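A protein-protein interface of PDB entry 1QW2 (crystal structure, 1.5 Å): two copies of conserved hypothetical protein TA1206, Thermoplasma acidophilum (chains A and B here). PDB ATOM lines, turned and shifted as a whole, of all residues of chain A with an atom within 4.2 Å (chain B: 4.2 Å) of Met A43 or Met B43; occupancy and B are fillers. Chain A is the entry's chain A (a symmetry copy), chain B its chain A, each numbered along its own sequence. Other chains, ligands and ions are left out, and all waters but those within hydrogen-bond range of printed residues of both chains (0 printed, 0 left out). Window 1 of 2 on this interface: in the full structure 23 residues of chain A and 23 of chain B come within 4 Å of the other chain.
The backbone carbonyl oxygen (O) of Tyr A46 sits close to the backbone carbonyl oxygen (O) of Tyr B46, 3.3 Å away.
The backbone NH of Met B43 lies within hydrogen-bond range of the backbone carbonyl oxygen of Val B60 (3.0 Å).
N of Val B62 sits at hydrogen-bond distance from O of Met B43 (3.0 Å).
SG of Cys B44 sits close to N of Tyr B46.
The backbone carbonyl oxygen (O) of Leu B47 is in hydrogen-bond range of the guanidinium group (NE) of Arg B61, 3.1 Å away.
The side-chain sulfur of Cys A44 sits close to the backbone NH of Tyr A46.
The backbone carbonyl oxygen (O) of Leu A47 lies within hydrogen-bond range of the guanidinium group (NE) of Arg A61, 3.1 Å away.
Hydrophobic or aromatic side chains of chain B within 4 Å of the printed part of chain A: Met B43, Tyr B46 and Leu B47.
Among the printed residues, 4 pairs touch across the chains.
Among the printed residues, no Asp or Glu carboxylate lies within 4 Å of a Lys or Arg side-chain nitrogen of the other chain.
Among the printed residues, pairs that only touch across the chains: Tyr A46 with Leu B47 (3.7 Å), Leu A47 with Tyr B46 (3.7 Å) and Met A43 with Met B43 (3.9 Å).
Met A43 touches just one residue of chain B: Met B43 (3.9 Å).
Of chain A, only Met A43 (3.9 Å) comes within 4 Å of Met B43.
Printed residues of chain B within 4 Å of Leu A47: Tyr B46 (3.7 Å).
Printed residues of chain B within 4 Å of Tyr A46: Tyr B46 and Leu B47.
Of the printed residues of chain A, Tyr B46 touches Tyr A46 and Leu A47.
Of the printed residues of chain A, Leu B47 touches Tyr A46 (3.7 Å).
Met A71 touches none of the printed residues of chain B.
The nearest printed residue of chain B that does not touch Leu A47 is Leu B47 (5.1 Å).
Met B43 touches its own counterpart, Met A43.
Tyr A46 touches its own counterpart, Tyr B46.
Tyr A46 touches Leu B47, and with the chains exchanged Leu A47 touches Tyr B46.
11 positions are printed for both chains.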
ATOM      1  N   LEU A  33     -25.856  18.669   9.012  1.00  0.00           N
ATOM      2  CA  LEU A  33     -26.453  19.961   8.744  1.00  0.00           C
ATOM      3  C   LEU A  33     -26.585  20.198   7.258  1.00  0.00           C
ATOM      4  O   LEU A  33     -25.756  19.752   6.464  1.00  0.00           O
ATOM      5  CB  LEU A  33     -25.665  21.103   9.404  1.00  0.00           C
ATOM      6  CG  LEU A  33     -24.178  21.313   9.152  1.00  0.00           C
ATOM      7  CD1 LEU A  33     -23.766  22.661   9.751  1.00  0.00           C
ATOM      8  CD2 LEU A  33     -23.374  20.177   9.778  1.00  0.00           C
ATOM      9  N   PHE A  34     -27.669  20.870   6.891  1.00  0.00           N
ATOM     10  CA  PHE A  34     -27.926  21.195   5.504  1.00  0.00           C
ATOM     11  C   PHE A  34     -28.735  22.476   5.391  1.00  0.00           C
ATOM     12  O   PHE A  34     -29.313  22.952   6.371  1.00  0.00           O
ATOM     13  CB  PHE A  34     -28.654  20.028   4.793  1.00  0.00           C
ATOM     14  CG  PHE A  34     -30.066  19.771   5.276  1.00  0.00           C
ATOM     15  CD1 PHE A  34     -31.117  20.615   4.911  1.00  0.00           C
ATOM     16  CD2 PHE A  34     -30.353  18.653   6.050  1.00  0.00           C
ATOM     17  CE1 PHE A  34     -32.432  20.344   5.308  1.00  0.00           C
ATOM     18  CE2 PHE A  34     -31.667  18.372   6.452  1.00  0.00           C
ATOM     19  CZ  PHE A  34     -32.704  19.218   6.079  1.00  0.00           C
ATOM     20  N   ALA A  42     -27.601  22.217   0.018  1.00  0.00           N
ATOM     21  CA  ALA A  42     -26.182  22.132   0.344  1.00  0.00           C
ATOM     22  C   ALA A  42     -26.145  21.311   1.624  1.00  0.00           C
ATOM     23  O   ALA A  42     -26.961  21.520   2.520  1.00  0.00           O
ATOM     24  CB  ALA A  42     -25.601  23.512   0.601  1.00  0.00           C
ATOM     25  N   MET A  43     -25.214  20.372   1.716  1.00  0.00           N
ATOM     26  CA  MET A  43     -25.128  19.551   2.912  1.00  0.00           C
ATOM     27  C   MET A  43     -23.676  19.319   3.299  1.00  0.00           C
ATOM     28  O   MET A  43     -22.773  19.444   2.468  1.00  0.00           O
ATOM     29  CB  MET A  43     -25.845  18.211   2.690  1.00  0.00           C
ATOM     30  CG  MET A  43     -25.961  17.342   3.932  1.00  0.00           C
ATOM     31  SD  MET A  43     -27.142  15.820   3.634  1.00  0.00           S
ATOM     32  CE  MET A  43     -26.206  14.514   4.671  1.00  0.00           C
ATOM     33  N   CYS A  44     -23.474  18.998   4.573  1.00  0.00           N
ATOM     34  CA  CYS A  44     -22.156  18.729   5.130  1.00  0.00           C
ATOM     35  C   CYS A  44     -21.561  17.449   4.545  1.00  0.00           C
ATOM     36  O   CYS A  44     -22.149  16.824   3.663  1.00  0.00           O
ATOM     37  CB  CYS A  44     -22.255  18.594   6.652  1.00  0.00           C
ATOM     38  SG  CYS A  44     -23.250  17.177   7.180  1.00  0.00           S
ATOM     39  N   TYR A  46     -21.515  14.437   5.364  1.00  0.00           N
ATOM     40  CA  TYR A  46     -22.272  13.192   5.389  1.00  0.00           C
ATOM     41  C   TYR A  46     -23.031  12.940   4.085  1.00  0.00           C
ATOM     42  O   TYR A  46     -23.526  11.835   3.858  1.00  0.00           O
ATOM     43  CB  TYR A  46     -23.250  13.180   6.567  1.00  0.00           C
ATOM     44  CG  TYR A  46     -22.630  12.814   7.901  1.00  0.00           C
ATOM     45  CD1 TYR A  46     -22.011  11.575   8.092  1.00  0.00           C
ATOM     46  CD2 TYR A  46     -22.712  13.684   8.986  1.00  0.00           C
ATOM     47  CE1 TYR A  46     -21.492  11.213   9.343  1.00  0.00           C
ATOM     48  CE2 TYR A  46     -22.198  13.334  10.236  1.00  0.00           C
ATOM     49  CZ  TYR A  46     -21.596  12.102  10.407  1.00  0.00           C
ATOM     50  OH  TYR A  46     -21.126  11.744  11.652  1.00  0.00           O
ATOM     51  N   LEU A  47     -23.106  13.947   3.219  1.00  0.00           N
ATOM     52  CA  LEU A  47     -23.809  13.778   1.951  1.00  0.00           C
ATOM     53  C   LEU A  47     -23.062  12.877   0.982  1.00  0.00           C
ATOM     54  O   LEU A  47     -21.857  13.023   0.777  1.00  0.00           O
ATOM     55  CB  LEU A  47     -24.046  15.129   1.269  1.00  0.00           C
ATOM     56  CG  LEU A  47     -24.702  15.040  -0.116  1.00  0.00           C
ATOM     57  CD1 LEU A  47     -26.115  14.501   0.021  1.00  0.00           C
ATOM     58  CD2 LEU A  47     -24.724  16.415  -0.774  1.00  0.00           C
ATOM     59  N   VAL A  60     -24.882  20.496  -3.501  1.00  0.00           N
ATOM     60  CA  VAL A  60     -23.486  20.816  -3.251  1.00  0.00           C
ATOM     61  C   VAL A  60     -23.104  20.231  -1.897  1.00  0.00           C
ATOM     62  O   VAL A  60     -23.917  20.173  -0.965  1.00  0.00           O
ATOM     63  CB  VAL A  60     -23.213  22.340  -3.263  1.00  0.00           C
ATOM     64  CG1 VAL A  60     -23.357  22.881  -4.681  1.00  0.00           C
ATOM     65  CG2 VAL A  60     -24.155  23.045  -2.326  1.00  0.00           C
ATOM     66  N   ARG A  61     -21.861  19.783  -1.803  1.00  0.00           N
ATOM     67  CA  ARG A  61     -21.345  19.186  -0.585  1.00  0.00           C
ATOM     68  C   ARG A  61     -20.202  20.052  -0.071  1.00  0.00           C
ATOM     69  O   ARG A  61     -19.331  20.451  -0.844  1.00  0.00           O
ATOM     70  CB  ARG A  61     -20.851  17.769  -0.897  1.00  0.00           C
ATOM     71  CG  ARG A  61     -20.247  17.009   0.272  1.00  0.00           C
ATOM     72  CD  ARG A  61     -20.057  15.537  -0.088  1.00  0.00           C
ATOM     73  NE  ARG A  61     -19.384  14.800   0.975  1.00  0.00           N
ATOM     74  CZ  ARG A  61     -18.070  14.615   1.044  1.00  0.00           C
ATOM     75  NH1 ARG A  61     -17.279  15.105   0.096  1.00  0.00           N
ATOM     76  NH2 ARG A  61     -17.544  13.964   2.072  1.00  0.00           N
ATOM     77  N   VAL A  62     -20.236  20.378   1.218  1.00  0.00           N
ATOM     78  CA  VAL A  62     -19.178  21.170   1.846  1.00  0.00           C
ATOM     79  C   VAL A  62     -18.654  20.330   3.003  1.00  0.00           C
ATOM     80  O   VAL A  62     -19.339  19.417   3.467  1.00  0.00           O
ATOM     81  CB  VAL A  62     -19.699  22.532   2.378  1.00  0.00           C
ATOM     82  CG1 VAL A  62     -20.130  23.410   1.215  1.00  0.00           C
ATOM     83  CG2 VAL A  62     -20.854  22.323   3.341  1.00  0.00           C
ATOM     84  N   MET A  71     -21.064  26.979   6.926  1.00  0.00           N
ATOM     85  CA  MET A  71     -21.532  26.510   5.626  1.00  0.00           C
ATOM     86  C   MET A  71     -21.512  27.596   4.562  1.00  0.00           C
ATOM     87  O   MET A  71     -21.028  27.378   3.454  1.00  0.00           O
ATOM     88  CB  MET A  71     -22.953  25.952   5.727  1.00  0.00           C
ATOM     89  CG  MET A  71     -23.053  24.601   6.393  1.00  0.00           C
ATOM     90  SD  MET A  71     -24.807  23.845   6.107  1.00  0.00           S
ATOM     91  CE  MET A  71     -24.562  23.176   4.333  1.00  0.00           C
ATOM     92  N   LEU B  33     -34.032  10.598   5.410  1.00  0.00           N
ATOM     93  CA  LEU B  33     -34.571  10.032   6.629  1.00  0.00           C
ATOM     94  C   LEU B  33     -33.529   9.213   7.353  1.00  0.00           C
ATOM     95  O   LEU B  33     -32.671   8.581   6.735  1.00  0.00           O
ATOM     96  CB  LEU B  33     -35.829   9.190   6.362  1.00  0.00           C
ATOM     97  CG  LEU B  33     -35.833   8.032   5.372  1.00  0.00           C
ATOM     98  CD1 LEU B  33     -37.147   7.261   5.529  1.00  0.00           C
ATOM     99  CD2 LEU B  33     -35.683   8.558   3.948  1.00  0.00           C
ATOM    100  N   PHE B  34     -33.588   9.272   8.677  1.00  0.00           N
ATOM    101  CA  PHE B  34     -32.671   8.524   9.511  1.00  0.00           C
ATOM    102  C   PHE B  34     -33.315   8.173  10.841  1.00  0.00           C
ATOM    103  O   PHE B  34     -34.352   8.729  11.213  1.00  0.00           O
ATOM    104  CB  PHE B  34     -31.361   9.320   9.735  1.00  0.00           C
ATOM    105  CG  PHE B  34     -31.516  10.578  10.564  1.00  0.00           C
ATOM    106  CD1 PHE B  34     -31.683  10.513  11.948  1.00  0.00           C
ATOM    107  CD2 PHE B  34     -31.437  11.829   9.965  1.00  0.00           C
ATOM    108  CE1 PHE B  34     -31.765  11.677  12.722  1.00  0.00           C
ATOM    109  CE2 PHE B  34     -31.518  13.002  10.730  1.00  0.00           C
ATOM    110  CZ  PHE B  34     -31.681  12.923  12.107  1.00  0.00           C
ATOM    111  N   ALA B  42     -28.952   4.918  11.612  1.00  0.00           N
ATOM    112  CA  ALA B  42     -29.234   4.276  10.333  1.00  0.00           C
ATOM    113  C   ALA B  42     -29.755   5.405   9.458  1.00  0.00           C
ATOM    114  O   ALA B  42     -30.549   6.227   9.911  1.00  0.00           O
ATOM    115  CB  ALA B  42     -30.304   3.209  10.486  1.00  0.00           C
ATOM    116  N   MET B  43     -29.307   5.463   8.212  1.00  0.00           N
ATOM    117  CA  MET B  43     -29.763   6.521   7.326  1.00  0.00           C
ATOM    118  C   MET B  43     -30.005   5.980   5.925  1.00  0.00           C
ATOM    119  O   MET B  43     -29.468   4.934   5.551  1.00  0.00           O
ATOM    120  CB  MET B  43     -28.737   7.663   7.289  1.00  0.00           C
ATOM    121  CG  MET B  43     -29.191   8.897   6.524  1.00  0.00           C
ATOM    122  SD  MET B  43     -27.970  10.393   6.788  1.00  0.00           S
ATOM    123  CE  MET B  43     -28.051  11.152   5.035  1.00  0.00           C
ATOM    124  N   CYS B  44     -30.832   6.700   5.176  1.00  0.00           N
ATOM    125  CA  CYS B  44     -31.180   6.349   3.805  1.00  0.00           C
ATOM    126  C   CYS B  44     -29.971   6.475   2.880  1.00  0.00           C
ATOM    127  O   CYS B  44     -28.861   6.767   3.325  1.00  0.00           O
ATOM    128  CB  CYS B  44     -32.301   7.264   3.305  1.00  0.00           C
ATOM    129  SG  CYS B  44     -31.809   9.003   3.199  1.00  0.00           S
ATOM    130  N   TYR B  46     -28.798   8.708   1.040  1.00  0.00           N
ATOM    131  CA  TYR B  46     -28.024   9.942   1.000  1.00  0.00           C
ATOM    132  C   TYR B  46     -26.796   9.895   1.913  1.00  0.00           C
ATOM    133  O   TYR B  46     -25.921  10.756   1.822  1.00  0.00           O
ATOM    134  CB  TYR B  46     -28.901  11.139   1.376  1.00  0.00           C
ATOM    135  CG  TYR B  46     -29.769  11.665   0.251  1.00  0.00           C
ATOM    136  CD1 TYR B  46     -29.203  12.146  -0.934  1.00  0.00           C
ATOM    137  CD2 TYR B  46     -31.154  11.732   0.393  1.00  0.00           C
ATOM    138  CE1 TYR B  46     -30.004  12.688  -1.948  1.00  0.00           C
ATOM    139  CE2 TYR B  46     -31.961  12.270  -0.611  1.00  0.00           C
ATOM    140  CZ  TYR B  46     -31.381  12.747  -1.772  1.00  0.00           C
ATOM    141  OH  TYR B  46     -32.177  13.313  -2.744  1.00  0.00           O
ATOM    142  N   LEU B  47     -26.715   8.884   2.774  1.00  0.00           N
ATOM    143  CA  LEU B  47     -25.570   8.770   3.671  1.00  0.00           C
ATOM    144  C   LEU B  47     -24.293   8.378   2.947  1.00  0.00           C
ATOM    145  O   LEU B  47     -24.282   7.454   2.132  1.00  0.00           O
ATOM    146  CB  LEU B  47     -25.835   7.740   4.774  1.00  0.00           C
ATOM    147  CG  LEU B  47     -24.648   7.489   5.714  1.00  0.00           C
ATOM    148  CD1 LEU B  47     -24.356   8.745   6.516  1.00  0.00           C
ATOM    149  CD2 LEU B  47     -24.957   6.327   6.650  1.00  0.00           C
ATOM    150  N   VAL B  60     -25.258   2.538   9.761  1.00  0.00           N
ATOM    151  CA  VAL B  60     -25.723   1.624   8.731  1.00  0.00           C
ATOM    152  C   VAL B  60     -26.463   2.437   7.677  1.00  0.00           C
ATOM    153  O   VAL B  60     -27.125   3.438   7.980  1.00  0.00           O
ATOM    154  CB  VAL B  60     -26.651   0.519   9.292  1.00  0.00           C
ATOM    155  CG1 VAL B  60     -25.847  -0.446  10.156  1.00  0.00           C
ATOM    156  CG2 VAL B  60     -27.774   1.133  10.083  1.00  0.00           C
ATOM    157  N   ARG B  61     -26.331   2.006   6.432  1.00  0.00           N
ATOM    158  CA  ARG B  61     -26.963   2.677   5.311  1.00  0.00           C
ATOM    159  C   ARG B  61     -27.955   1.715   4.670  1.00  0.00           C
ATOM    160  O   ARG B  61     -27.629   0.550   4.440  1.00  0.00           O
ATOM    161  CB  ARG B  61     -25.882   3.087   4.305  1.00  0.00           C
ATOM    162  CG  ARG B  61     -26.381   3.780   3.047  1.00  0.00           C
ATOM    163  CD  ARG B  61     -25.213   4.384   2.270  1.00  0.00           C
ATOM    164  NE  ARG B  61     -25.645   4.967   1.005  1.00  0.00           N
ATOM    165  CZ  ARG B  61     -25.656   4.319  -0.155  1.00  0.00           C
ATOM    166  NH1 ARG B  61     -25.242   3.059  -0.216  1.00  0.00           N
ATOM    167  NH2 ARG B  61     -26.106   4.921  -1.248  1.00  0.00           N
ATOM    168  N   VAL B  62     -29.174   2.190   4.430  1.00  0.00           N
ATOM    169  CA  VAL B  62     -30.208   1.382   3.782  1.00  0.00           C
ATOM    170  C   VAL B  62     -30.644   2.166   2.552  1.00  0.00           C
ATOM    171  O   VAL B  62     -30.423   3.376   2.477  1.00  0.00           O
ATOM    172  CB  VAL B  62     -31.428   1.133   4.708  1.00  0.00           C
ATOM    173  CG1 VAL B  62     -31.015   0.267   5.886  1.00  0.00           C
ATOM    174  CG2 VAL B  62     -32.005   2.450   5.196  1.00  0.00           C
ATOM    175  N   MET B  71     -37.662   1.545   6.523  1.00  0.00           N
ATOM    176  CA  MET B  71     -36.322   1.456   7.092  1.00  0.00           C
ATOM    177  C   MET B  71     -36.136   0.239   7.985  1.00  0.00           C
ATOM    178  O   MET B  71     -35.150  -0.483   7.861  1.00  0.00           O
ATOM    179  CB  MET B  71     -35.990   2.710   7.903  1.00  0.00           C
ATOM    180  CG  MET B  71     -35.694   3.936   7.073  1.00  0.00           C
ATOM    181  SD  MET B  71     -34.918   5.318   8.178  1.00  0.00           S
ATOM    182  CE  MET B  71     -33.117   4.678   8.239  1.00  0.00           C
